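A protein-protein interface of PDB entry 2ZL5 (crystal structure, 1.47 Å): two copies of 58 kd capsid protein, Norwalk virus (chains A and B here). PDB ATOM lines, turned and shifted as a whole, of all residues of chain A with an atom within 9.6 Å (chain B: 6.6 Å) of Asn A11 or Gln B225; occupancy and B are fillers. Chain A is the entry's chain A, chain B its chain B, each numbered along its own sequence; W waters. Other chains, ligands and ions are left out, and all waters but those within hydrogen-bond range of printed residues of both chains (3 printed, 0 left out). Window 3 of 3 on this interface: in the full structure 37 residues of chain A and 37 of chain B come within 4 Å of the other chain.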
ATOM      1  N   THR A   8      -0.534   9.235 -31.488  1.00  0.00           N
ATOM      2  CA  THR A   8       0.015   9.779 -30.250  1.00  0.00           C
ATOM      3  C   THR A   8      -0.339   8.970 -28.998  1.00  0.00           C
ATOM      4  O   THR A   8      -1.398   8.350 -28.908  1.00  0.00           O
ATOM      5  CB  THR A   8      -0.437  11.233 -29.985  1.00  0.00           C
ATOM      6  OG1 THR A   8      -1.844  11.244 -29.776  1.00  0.00           O
ATOM      7  CG2 THR A   8      -0.097  12.173 -31.136  1.00  0.00           C
ATOM      8  N   LEU A   9       0.568   9.034 -28.030  1.00  0.00           N
ATOM      9  CA  LEU A   9       0.305   8.666 -26.640  1.00  0.00           C
ATOM     10  C   LEU A   9       0.308   9.943 -25.798  1.00  0.00           C
ATOM     11  O   LEU A   9       0.871  10.968 -26.218  1.00  0.00           O
ATOM     12  CB  LEU A   9       1.394   7.731 -26.111  1.00  0.00           C
ATOM     13  CG  LEU A   9       1.456   6.404 -26.861  1.00  0.00           C
ATOM     14  CD1 LEU A   9       2.638   5.650 -26.339  1.00  0.00           C
ATOM     15  CD2 LEU A   9       0.189   5.594 -26.609  1.00  0.00           C
ATOM     16  N   PRO A  10      -0.291   9.906 -24.598  1.00  0.00           N
ATOM     17  CA  PRO A  10      -0.335  11.146 -23.792  1.00  0.00           C
ATOM     18  C   PRO A  10       1.039  11.727 -23.521  1.00  0.00           C
ATOM     19  O   PRO A  10       1.983  10.990 -23.205  1.00  0.00           O
ATOM     20  CB  PRO A  10      -0.917  10.662 -22.457  1.00  0.00           C
ATOM     21  CG  PRO A  10      -1.801   9.496 -22.871  1.00  0.00           C
ATOM     22  CD  PRO A  10      -1.041   8.803 -23.956  1.00  0.00           C
ATOM     23  N   ASN A  11       1.141  13.039 -23.696  1.00  0.00           N
ATOM     24  CA  ASN A  11       2.376  13.746 -23.373  1.00  0.00           C
ATOM     25  C   ASN A  11       2.334  14.140 -21.901  1.00  0.00           C
ATOM     26  O   ASN A  11       2.209  15.323 -21.560  1.00  0.00           O
ATOM     27  CB  ASN A  11       2.542  14.970 -24.282  1.00  0.00           C
ATOM     28  CG  ASN A  11       3.819  15.743 -23.993  1.00  0.00           C
ATOM     29  OD1 ASN A  11       4.777  15.197 -23.453  1.00  0.00           O
ATOM     30  ND2 ASN A  11       3.797  17.045 -24.292  1.00  0.00           N
ATOM     31  N   LEU A  12       2.396  13.124 -21.032  1.00  0.00           N
ATOM     32  CA  LEU A  12       2.264  13.268 -19.581  1.00  0.00           C
ATOM     33  C   LEU A  12       3.228  12.288 -18.915  1.00  0.00           C
ATOM     34  O   LEU A  12       3.330  11.132 -19.348  1.00  0.00           O
ATOM     35  CB  LEU A  12       0.841  12.887 -19.184  1.00  0.00           C
ATOM     36  CG  LEU A  12      -0.249  13.816 -19.703  1.00  0.00           C
ATOM     37  CD1 LEU A  12      -1.629  13.176 -19.488  1.00  0.00           C
ATOM     38  CD2 LEU A  12      -0.155  15.202 -19.054  1.00  0.00           C
ATOM     39  N   PRO A  13       3.897  12.696 -17.852  1.00  0.00           N
ATOM     40  CA  PRO A  13       4.837  11.759 -17.198  1.00  0.00           C
ATOM     41  C   PRO A  13       4.083  10.626 -16.506  1.00  0.00           C
ATOM     42  O   PRO A  13       2.982  10.832 -15.961  1.00  0.00           O
ATOM     43  CB  PRO A  13       5.569  12.621 -16.172  1.00  0.00           C
ATOM     44  CG  PRO A  13       4.678  13.772 -15.931  1.00  0.00           C
ATOM     45  CD  PRO A  13       3.845  14.002 -17.181  1.00  0.00           C
ATOM     46  N   LEU A  14       4.672   9.431 -16.503  1.00  0.00           N
ATOM     47  CA  LEU A  14       3.968   8.262 -15.952  1.00  0.00           C
ATOM     48  C   LEU A  14       3.540   8.453 -14.513  1.00  0.00           C
ATOM     49  O   LEU A  14       2.459   8.028 -14.113  1.00  0.00           O
ATOM     50  CB  LEU A  14       4.819   6.975 -16.093  1.00  0.00           C
ATOM     51  CG  LEU A  14       5.102   6.599 -17.537  1.00  0.00           C
ATOM     52  CD1 LEU A  14       5.930   5.321 -17.552  1.00  0.00           C
ATOM     53  CD2 LEU A  14       3.798   6.400 -18.355  1.00  0.00           C
ATOM     54  N   SER A  16       2.461  10.890 -13.043  1.00  0.00           N
ATOM     55  CA  SER A  16       1.250  11.715 -12.901  1.00  0.00           C
ATOM     56  C   SER A  16      -0.026  10.946 -13.232  1.00  0.00           C
ATOM     57  O   SER A  16      -1.112  11.520 -13.171  1.00  0.00           O
ATOM     58  CB  SER A  16       1.320  12.939 -13.816  1.00  0.00           C
ATOM     59  OG  SER A  16       2.379  13.789 -13.415  1.00  0.00           O
ATOM     60  N   LEU A  17       0.113   9.675 -13.613  1.00  0.00           N
ATOM     61  CA  LEU A  17      -1.022   8.901 -14.168  1.00  0.00           C
ATOM     62  C   LEU A  17      -1.523   7.849 -13.187  1.00  0.00           C
ATOM     63  O   LEU A  17      -0.952   7.667 -12.106  1.00  0.00           O
ATOM     64  CB  LEU A  17      -0.629   8.277 -15.506  1.00  0.00           C
ATOM     65  CG  LEU A  17      -0.080   9.303 -16.508  1.00  0.00           C
ATOM     66  CD1 LEU A  17       0.229   8.575 -17.811  1.00  0.00           C
ATOM     67  CD2 LEU A  17      -1.039  10.470 -16.749  1.00  0.00           C
ATOM     68  N   GLU A 216      -5.120   6.888 -18.113  1.00  0.00           N
ATOM     69  CA  GLU A 216      -5.152   8.048 -19.003  1.00  0.00           C
ATOM     70  C   GLU A 216      -4.743   7.709 -20.429  1.00  0.00           C
ATOM     71  O   GLU A 216      -5.125   8.379 -21.391  1.00  0.00           O
ATOM     72  CB  GLU A 216      -4.315   9.212 -18.437  1.00  0.00           C
ATOM     73  CG  GLU A 216      -4.930   9.838 -17.147  1.00  0.00           C
ATOM     74  CD  GLU A 216      -4.703   9.002 -15.906  1.00  0.00           C
ATOM     75  OE1 GLU A 216      -3.915   8.020 -15.950  1.00  0.00           O
ATOM     76  OE2 GLU A 216      -5.353   9.324 -14.882  1.00  0.00           O
ATOM     77  N   TYR A 217      -3.972   6.627 -20.579  1.00  0.00           N
ATOM     78  CA  TYR A 217      -3.672   6.166 -21.934  1.00  0.00           C
ATOM     79  C   TYR A 217      -4.930   5.586 -22.597  1.00  0.00           C
ATOM     80  O   TYR A 217      -5.144   5.759 -23.798  1.00  0.00           O
ATOM     81  CB  TYR A 217      -2.601   5.062 -21.908  1.00  0.00           C
ATOM     82  CG  TYR A 217      -1.157   5.529 -21.863  1.00  0.00           C
ATOM     83  CD1 TYR A 217      -0.764   6.612 -21.082  1.00  0.00           C
ATOM     84  CD2 TYR A 217      -0.199   4.877 -22.616  1.00  0.00           C
ATOM     85  CE1 TYR A 217       0.571   7.006 -21.020  1.00  0.00           C
ATOM     86  CE2 TYR A 217       1.130   5.260 -22.574  1.00  0.00           C
ATOM     87  CZ  TYR A 217       1.497   6.339 -21.789  1.00  0.00           C
ATOM     88  OH  TYR A 217       2.823   6.741 -21.766  1.00  0.00           O
ATOM     89  N   HIS A 220      -7.158   8.340 -23.669  1.00  0.00           N
ATOM     90  CA  HIS A 220      -6.504   8.969 -24.817  1.00  0.00           C
ATOM     91  C   HIS A 220      -6.736   8.154 -26.087  1.00  0.00           C
ATOM     92  O   HIS A 220      -7.135   8.700 -27.111  1.00  0.00           O
ATOM     93  CB  HIS A 220      -5.004   9.134 -24.544  1.00  0.00           C
ATOM     94  CG  HIS A 220      -4.286   9.899 -25.601  1.00  0.00           C
ATOM     95  ND1 HIS A 220      -3.735   9.314 -26.730  1.00  0.00           N
ATOM     96  CD2 HIS A 220      -4.023  11.222 -25.691  1.00  0.00           C
ATOM     97  CE1 HIS A 220      -3.181  10.261 -27.475  1.00  0.00           C
ATOM     98  NE2 HIS A 220      -3.328  11.418 -26.862  1.00  0.00           N
ATOM     99  N   GLU A 224      -8.810   9.206 -29.403  1.00  0.00           N
ATOM    100  CA  GLU A 224      -8.051   9.391 -30.643  1.00  0.00           C
ATOM    101  C   GLU A 224      -8.562   8.526 -31.802  1.00  0.00           C
ATOM    102  O   GLU A 224      -8.561   8.948 -32.972  1.00  0.00           O
ATOM    103  CB  GLU A 224      -6.577   9.093 -30.345  1.00  0.00           C
ATOM    104  CG  GLU A 224      -5.638   9.013 -31.559  1.00  0.00           C
ATOM    105  CD  GLU A 224      -4.185   8.695 -31.201  1.00  0.00           C
ATOM    106  OE1 GLU A 224      -3.903   8.286 -30.041  1.00  0.00           O
ATOM    107  OE2 GLU A 224      -3.309   8.833 -32.095  1.00  0.00           O
ATOM    108  N   HIS A 236       9.930   5.894 -27.823  1.00  0.00           N
ATOM    109  CA  HIS A 236      11.013   6.183 -26.885  1.00  0.00           C
ATOM    110  C   HIS A 236      10.434   6.583 -25.539  1.00  0.00           C
ATOM    111  O   HIS A 236       9.427   7.315 -25.478  1.00  0.00           O
ATOM    112  CB  HIS A 236      11.899   7.336 -27.397  1.00  0.00           C
ATOM    113  CG  HIS A 236      12.706   6.997 -28.616  1.00  0.00           C
ATOM    114  ND1 HIS A 236      13.309   7.959 -29.400  1.00  0.00           N
ATOM    115  CD2 HIS A 236      12.986   5.805 -29.201  1.00  0.00           C
ATOM    116  CE1 HIS A 236      13.932   7.372 -30.409  1.00  0.00           C
ATOM    117  NE2 HIS A 236      13.765   6.066 -30.305  1.00  0.00           N
ATOM    118  N   VAL A 238      11.146   9.011 -22.778  1.00  0.00           N
ATOM    119  CA  VAL A 238      11.913  10.264 -22.826  1.00  0.00           C
ATOM    120  C   VAL A 238      11.884  10.982 -21.485  1.00  0.00           C
ATOM    121  O   VAL A 238      10.826  11.081 -20.821  1.00  0.00           O
ATOM    122  CB  VAL A 238      11.367  11.188 -23.924  1.00  0.00           C
ATOM    123  CG1 VAL A 238      12.157  12.500 -24.014  1.00  0.00           C
ATOM    124  CG2 VAL A 238      11.407  10.472 -25.274  1.00  0.00           C
ATOM    125  N   ASP A 239      13.036  11.521 -21.095  1.00  0.00           N
ATOM    126  CA  ASP A 239      13.084  12.485 -20.010  1.00  0.00           C
ATOM    127  C   ASP A 239      12.720  13.870 -20.559  1.00  0.00           C
ATOM    128  O   ASP A 239      13.402  14.383 -21.439  1.00  0.00           O
ATOM    129  CB  ASP A 239      14.470  12.516 -19.373  1.00  0.00           C
ATOM    130  CG  ASP A 239      14.592  13.619 -18.347  1.00  0.00           C
ATOM    131  OD1 ASP A 239      13.920  13.528 -17.307  1.00  0.00           O
ATOM    132  OD2 ASP A 239      15.340  14.593 -18.596  1.00  0.00           O
ATOM    133  N   PRO A 240      11.604  14.464 -20.085  1.00  0.00           N
ATOM    134  CA  PRO A 240      11.096  15.722 -20.659  1.00  0.00           C
ATOM    135  C   PRO A 240      12.082  16.905 -20.709  1.00  0.00           C
ATOM    136  O   PRO A 240      12.203  17.573 -21.758  1.00  0.00           O
ATOM    137  CB  PRO A 240       9.913  16.070 -19.737  1.00  0.00           C
ATOM    138  CG  PRO A 240       9.480  14.784 -19.205  1.00  0.00           C
ATOM    139  CD  PRO A 240      10.726  13.967 -19.011  1.00  0.00           C
ATOM    140  N   ASP A 241      12.772  17.148 -19.601  1.00  0.00           N
ATOM    141  CA  ASP A 241      13.684  18.306 -19.479  1.00  0.00           C
ATOM    142  C   ASP A 241      14.902  18.236 -20.392  1.00  0.00           C
ATOM    143  O   ASP A 241      15.235  19.223 -21.077  1.00  0.00           O
ATOM    144  CB  ASP A 241      14.158  18.490 -18.038  1.00  0.00           C
ATOM    145  CG  ASP A 241      13.095  19.101 -17.144  1.00  0.00           C
ATOM    146  OD1 ASP A 241      12.440  20.079 -17.575  1.00  0.00           O
ATOM    147  OD2 ASP A 241      12.923  18.596 -16.010  1.00  0.00           O
ATOM    148  N   ASN A 274       9.263   9.362 -14.041  1.00  0.00           N
ATOM    149  CA  ASN A 274       8.797  10.677 -14.467  1.00  0.00           C
ATOM    150  C   ASN A 274       8.994  10.948 -15.958  1.00  0.00           C
ATOM    151  O   ASN A 274       8.964  12.097 -16.400  1.00  0.00           O
ATOM    152  CB  ASN A 274       9.418  11.794 -13.611  1.00  0.00           C
ATOM    153  CG  ASN A 274      10.911  11.915 -13.820  1.00  0.00           C
ATOM    154  OD1 ASN A 274      11.560  11.024 -14.398  1.00  0.00           O
ATOM    155  ND2 ASN A 274      11.472  13.046 -13.378  1.00  0.00           N
ATOM    156  N   GLY A 275       9.215   9.891 -16.743  1.00  0.00           N
ATOM    157  CA  GLY A 275       9.385  10.043 -18.170  1.00  0.00           C
ATOM    158  C   GLY A 275       8.070   9.955 -18.938  1.00  0.00           C
ATOM    159  O   GLY A 275       7.005   9.664 -18.366  1.00  0.00           O
ATOM    160  N   VAL A 276       8.172  10.152 -20.236  1.00  0.00           N
ATOM    161  CA  VAL A 276       7.021  10.229 -21.116  1.00  0.00           C
ATOM    162  C   VAL A 276       7.252   9.284 -22.283  1.00  0.00           C
ATOM    163  O   VAL A 276       8.330   9.308 -22.893  1.00  0.00           O
ATOM    164  CB  VAL A 276       6.860  11.692 -21.643  1.00  0.00           C
ATOM    165  CG1 VAL A 276       5.845  11.789 -22.768  1.00  0.00           C
ATOM    166  CG2 VAL A 276       6.522  12.656 -20.501  1.00  0.00           C
ATOM    167  N   PHE A 277       6.286   8.422 -22.603  1.00  0.00           N
ATOM    168  CA  PHE A 277       6.397   7.637 -23.834  1.00  0.00           C
ATOM    169  C   PHE A 277       6.011   8.468 -25.032  1.00  0.00           C
ATOM    170  O   PHE A 277       4.948   9.121 -25.031  1.00  0.00           O
ATOM    171  CB  PHE A 277       5.529   6.378 -23.801  1.00  0.00           C
ATOM    172  CG  PHE A 277       6.124   5.266 -22.999  1.00  0.00           C
ATOM    173  CD1 PHE A 277       7.274   4.615 -23.451  1.00  0.00           C
ATOM    174  CD2 PHE A 277       5.552   4.877 -21.795  1.00  0.00           C
ATOM    175  CE1 PHE A 277       7.821   3.597 -22.719  1.00  0.00           C
ATOM    176  CE2 PHE A 277       6.103   3.854 -21.049  1.00  0.00           C
ATOM    177  CZ  PHE A 277       7.259   3.217 -21.524  1.00  0.00           C
ATOM    178  N   VAL A 278       6.845   8.422 -26.066  1.00  0.00           N
ATOM    179  CA  VAL A 278       6.653   9.216 -27.268  1.00  0.00           C
ATOM    180  C   VAL A 278       6.675   8.300 -28.474  1.00  0.00           C
ATOM    181  O   VAL A 278       7.630   7.532 -28.658  1.00  0.00           O
ATOM    182  CB  VAL A 278       7.781  10.287 -27.447  1.00  0.00           C
ATOM    183  CG1 VAL A 278       7.559  11.101 -28.713  1.00  0.00           C
ATOM    184  CG2 VAL A 278       7.880  11.185 -26.227  1.00  0.00           C
ATOM    185  N   PHE A 279       5.631   8.382 -29.290  1.00  0.00           N
ATOM    186  CA  PHE A 279       5.571   7.618 -30.525  1.00  0.00           C
ATOM    187  C   PHE A 279       6.662   8.100 -31.481  1.00  0.00           C
ATOM    188  O   PHE A 279       6.815   9.317 -31.694  1.00  0.00           O
ATOM    189  CB  PHE A 279       4.193   7.782 -31.165  1.00  0.00           C
ATOM    190  CG  PHE A 279       4.087   7.159 -32.529  1.00  0.00           C
ATOM    191  CD1 PHE A 279       4.055   5.770 -32.688  1.00  0.00           C
ATOM    192  CD2 PHE A 279       3.999   7.967 -33.675  1.00  0.00           C
ATOM    193  CE1 PHE A 279       3.954   5.200 -33.956  1.00  0.00           C
ATOM    194  CE2 PHE A 279       3.894   7.406 -34.952  1.00  0.00           C
ATOM    195  CZ  PHE A 279       3.852   6.012 -35.083  1.00  0.00           C
ATOM    196  N   LEU B  48      -7.105  26.278 -21.456  1.00  0.00           N
ATOM    197  CA  LEU B  48      -7.175  25.577 -22.738  1.00  0.00           C
ATOM    198  C   LEU B  48      -5.818  25.174 -23.306  1.00  0.00           C
ATOM    199  O   LEU B  48      -5.745  24.228 -24.104  1.00  0.00           O
ATOM    200  CB  LEU B  48      -7.972  26.385 -23.783  1.00  0.00           C
ATOM    201  CG  LEU B  48      -9.445  26.593 -23.424  1.00  0.00           C
ATOM    202  CD1 LEU B  48     -10.169  27.298 -24.585  1.00  0.00           C
ATOM    203  CD2 LEU B  48     -10.166  25.292 -23.039  1.00  0.00           C
ATOM    204  N   ASP B  49      -4.754  25.890 -22.908  1.00  0.00           N
ATOM    205  CA  ASP B  49      -3.403  25.531 -23.333  1.00  0.00           C
ATOM    206  C   ASP B  49      -2.718  24.499 -22.405  1.00  0.00           C
ATOM    207  O   ASP B  49      -1.539  24.196 -22.601  1.00  0.00           O
ATOM    208  CB  ASP B  49      -2.506  26.764 -23.610  1.00  0.00           C
ATOM    209  CG  ASP B  49      -2.086  27.512 -22.337  1.00  0.00           C
ATOM    210  OD1 ASP B  49      -2.390  27.088 -21.207  1.00  0.00           O
ATOM    211  OD2 ASP B  49      -1.421  28.544 -22.501  1.00  0.00           O
ATOM    212  N   GLY B  50      -3.442  23.991 -21.404  1.00  0.00           N
ATOM    213  CA  GLY B  50      -2.906  22.918 -20.583  1.00  0.00           C
ATOM    214  C   GLY B  50      -2.280  23.302 -19.266  1.00  0.00           C
ATOM    215  O   GLY B  50      -1.600  22.465 -18.692  1.00  0.00           O
ATOM    216  N   SER B 219      -6.799  16.016 -18.339  1.00  0.00           N
ATOM    217  CA  SER B 219      -5.630  15.272 -18.786  1.00  0.00           C
ATOM    218  C   SER B 219      -5.419  15.448 -20.289  1.00  0.00           C
ATOM    219  O   SER B 219      -4.276  15.558 -20.729  1.00  0.00           O
ATOM    220  CB  SER B 219      -5.708  13.798 -18.388  1.00  0.00           C
ATOM    221  OG  SER B 219      -6.917  13.210 -18.828  1.00  0.00           O
ATOM    222  N   HIS B 220      -6.507  15.526 -21.062  1.00  0.00           N
ATOM    223  CA  HIS B 220      -6.370  15.794 -22.497  1.00  0.00           C
ATOM    224  C   HIS B 220      -5.698  17.133 -22.766  1.00  0.00           C
ATOM    225  O   HIS B 220      -4.768  17.221 -23.553  1.00  0.00           O
ATOM    226  CB  HIS B 220      -7.757  15.777 -23.169  1.00  0.00           C
ATOM    227  CG  HIS B 220      -7.721  15.952 -24.655  1.00  0.00           C
ATOM    228  ND1 HIS B 220      -7.694  14.876 -25.524  1.00  0.00           N
ATOM    229  CD2 HIS B 220      -7.762  17.066 -25.431  1.00  0.00           C
ATOM    230  CE1 HIS B 220      -7.671  15.325 -26.766  1.00  0.00           C
ATOM    231  NE2 HIS B 220      -7.707  16.646 -26.739  1.00  0.00           N
ATOM    232  N   LEU B 221      -6.182  18.184 -22.096  1.00  0.00           N
ATOM    233  CA  LEU B 221      -5.619  19.525 -22.363  1.00  0.00           C
ATOM    234  C   LEU B 221      -4.186  19.630 -21.872  1.00  0.00           C
ATOM    235  O   LEU B 221      -3.362  20.314 -22.505  1.00  0.00           O
ATOM    236  CB  LEU B 221      -6.474  20.604 -21.694  1.00  0.00           C
ATOM    237  CG  LEU B 221      -7.874  20.799 -22.278  1.00  0.00           C
ATOM    238  CD1 LEU B 221      -8.741  21.665 -21.349  1.00  0.00           C
ATOM    239  CD2 LEU B 221      -7.827  21.390 -23.682  1.00  0.00           C
ATOM    240  N   ALA B 222      -3.892  18.982 -20.731  1.00  0.00           N
ATOM    241  CA  ALA B 222      -2.522  19.001 -20.159  1.00  0.00           C
ATOM    242  C   ALA B 222      -1.556  18.264 -21.067  1.00  0.00           C
ATOM    243  O   ALA B 222      -0.362  18.585 -21.092  1.00  0.00           O
ATOM    244  CB  ALA B 222      -2.484  18.411 -18.748  1.00  0.00           C
ATOM    245  N   SER B 223      -2.062  17.264 -21.785  1.00  0.00           N
ATOM    246  CA  SER B 223      -1.247  16.510 -22.713  1.00  0.00           C
ATOM    247  C   SER B 223      -1.064  17.299 -23.995  1.00  0.00           C
ATOM    248  O   SER B 223       0.041  17.404 -24.525  1.00  0.00           O
ATOM    249  CB  SER B 223      -1.905  15.155 -23.003  1.00  0.00           C
ATOM    250  OG  SER B 223      -1.287  14.499 -24.098  1.00  0.00           O
ATOM    251  N   GLU B 224      -2.165  17.831 -24.528  1.00  0.00           N
ATOM    252  CA  GLU B 224      -2.141  18.482 -25.834  1.00  0.00           C
ATOM    253  C   GLU B 224      -1.294  19.751 -25.852  1.00  0.00           C
ATOM    254  O   GLU B 224      -0.594  20.021 -26.853  1.00  0.00           O
ATOM    255  CB  GLU B 224      -3.589  18.777 -26.236  1.00  0.00           C
ATOM    256  CG  GLU B 224      -3.808  19.649 -27.446  1.00  0.00           C
ATOM    257  CD  GLU B 224      -5.297  19.941 -27.727  1.00  0.00           C
ATOM    258  OE1 GLU B 224      -6.194  19.638 -26.885  1.00  0.00           O
ATOM    259  OE2 GLU B 224      -5.567  20.528 -28.793  1.00  0.00           O
ATOM    260  N   GLN B 225      -1.367  20.532 -24.770  1.00  0.00           N
ATOM    261  CA  GLN B 225      -0.555  21.755 -24.640  1.00  0.00           C
ATOM    262  C   GLN B 225      -0.703  22.651 -25.879  1.00  0.00           C
ATOM    263  O   GLN B 225       0.299  23.133 -26.417  1.00  0.00           O
ATOM    264  CB  GLN B 225       0.910  21.409 -24.327  1.00  0.00           C
ATOM    265  CG  GLN B 225       1.051  20.708 -22.971  1.00  0.00           C
ATOM    266  CD  GLN B 225       2.410  20.109 -22.727  1.00  0.00           C
ATOM    267  OE1 GLN B 225       3.423  20.581 -23.263  1.00  0.00           O
ATOM    268  NE2 GLN B 225       2.440  19.049 -21.917  1.00  0.00           N
ATOM    269  N   ALA B 226      -1.943  22.850 -26.327  1.00  0.00           N
ATOM    270  CA  ALA B 226      -2.244  23.587 -27.559  1.00  0.00           C
ATOM    271  C   ALA B 226      -1.436  24.878 -27.686  1.00  0.00           C
ATOM    272  O   ALA B 226      -1.478  25.732 -26.796  1.00  0.00           O
ATOM    273  CB  ALA B 226      -3.729  23.877 -27.643  1.00  0.00           C
ATOM    274  N   PRO B 227      -0.678  25.008 -28.790  1.00  0.00           N
ATOM    275  CA  PRO B 227       0.139  26.192 -29.065  1.00  0.00           C
ATOM    276  C   PRO B 227      -0.637  27.374 -29.670  1.00  0.00           C
ATOM    277  O   PRO B 227      -0.085  28.468 -29.746  1.00  0.00           O
ATOM    278  CB  PRO B 227       1.198  25.663 -30.050  1.00  0.00           C
ATOM    279  CG  PRO B 227       0.544  24.524 -30.760  1.00  0.00           C
ATOM    280  CD  PRO B 227      -0.541  23.972 -29.838  1.00  0.00           C
ATOM    281  N   THR B 228      -1.897  27.174 -30.069  1.00  0.00           N
ATOM    282  CA  THR B 228      -2.629  28.201 -30.851  1.00  0.00           C
ATOM    283  C   THR B 228      -4.033  28.593 -30.319  1.00  0.00           C
ATOM    284  O   THR B 228      -4.980  28.812 -31.101  1.00  0.00           O
ATOM    285  CB  THR B 228      -2.687  27.834 -32.383  1.00  0.00           C
ATOM    286  OG1 THR B 228      -1.383  27.444 -32.841  1.00  0.00           O
ATOM    287  CG2 THR B 228      -3.170  29.020 -33.229  1.00  0.00           C
ATOM    288  N   ILE B 229      -4.156  28.727 -29.001  1.00  0.00           N
ATOM    289  CA  ILE B 229      -5.411  29.173 -28.366  1.00  0.00           C
ATOM    290  C   ILE B 229      -5.803  30.603 -28.751  1.00  0.00           C
ATOM    291  O   ILE B 229      -4.998  31.519 -28.583  1.00  0.00           O
ATOM    292  CB  ILE B 229      -5.284  29.092 -26.819  1.00  0.00           C
ATOM    293  CG1 ILE B 229      -4.780  27.705 -26.401  1.00  0.00           C
ATOM    294  CG2 ILE B 229      -6.603  29.526 -26.098  1.00  0.00           C
ATOM    295  CD1 ILE B 229      -5.782  26.595 -26.444  1.00  0.00           C
HETATM  296  O   HOH W   1       3.534  16.891 -19.665  1.00  0.00           O
HETATM  297  O   HOH W   2       2.012  17.834 -26.401  1.00  0.00           O
HETATM  298  O   HOH W   3       5.590  19.189 -23.481  1.00  0.00           O
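Water W3 lies within hydrogen-bond range of OE1 of Gln B225 (2.6 Å) and ND2 of Asn A11 (2.9 Å).
Water W2 lies within hydrogen-bond range of O of Ser B223 (2.8 Å), ND2 of Asn A11 (2.9 Å) and O of Glu B224 (3.4 Å).
Water W1 lies within hydrogen-bond range of the backbone carbonyl oxygen of Asn A11 (2.8 Å) and the side-chain amide nitrogen of Gln B225 (3.3 Å).
Asn A11 touches just these residues of chain B: Ser B223 (2.9 Å) and Gln B225 (3.4 Å).
Ser B223 touches just these residues of chain A: Pro A10 (3.5 Å), Asn A11 (2.9 Å) and Leu A12 (3.9 Å).
Of the printed residues of chain B, Leu A12 touches Ser B219 (3.8 Å), Ala B222 (3.9 Å) and Ser B223 (3.9 Å).
Of the printed residues of chain B, Pro A10 touches Ser B223.
Of the printed residues of chain A, Ala B222 touches Leu A12.
Of the printed residues of chain A, Ser B219 touches Leu A12.
Printed residues of chain A that touch a printed residue of chain B: Pro A10, Asn A11 and Leu A12.
Hydrophobic or aromatic side chains of chain A that line the printed part of chain B: Leu A12.
Printed residues of chain B that touch a printed residue of chain A: Ser B219, Ala B222, Ser B223 and Gln B225.
Hydrophobic or aromatic side chains of chain B that line the printed part of chain A: Ala B222.
Among the printed residues, no Asp or Glu carboxylate lies within 4 Å of a Lys or Arg side-chain nitrogen of the other chain.
OG of Ser B223 touches CA of Pro A10, 3.5 Å away.
CD1 of Leu A12 touches O of Ser B219, 3.8 Å away.
Leu A12 touches Ala B222.
Leu A12 touches Ser B223.
The side-chain amide nitrogen (NE2) of Gln B225 lies within hydrogen-bond range of the backbone carbonyl oxygen (O) of Ala B222, at 3.0 Å.
Positions printed for both chains: 220 and 224.
Of the 6 pairs that touch across the chains among the printed residues, none has its exchanged pair printed and touching as well.
The side-chain hydroxyl (OG) of Ser B223 lies within hydrogen-bond range of the backbone NH (N) of Asn A11, at 2.9 Å.
ND2 of Asn A11 sits close to NE2 of Gln B225.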
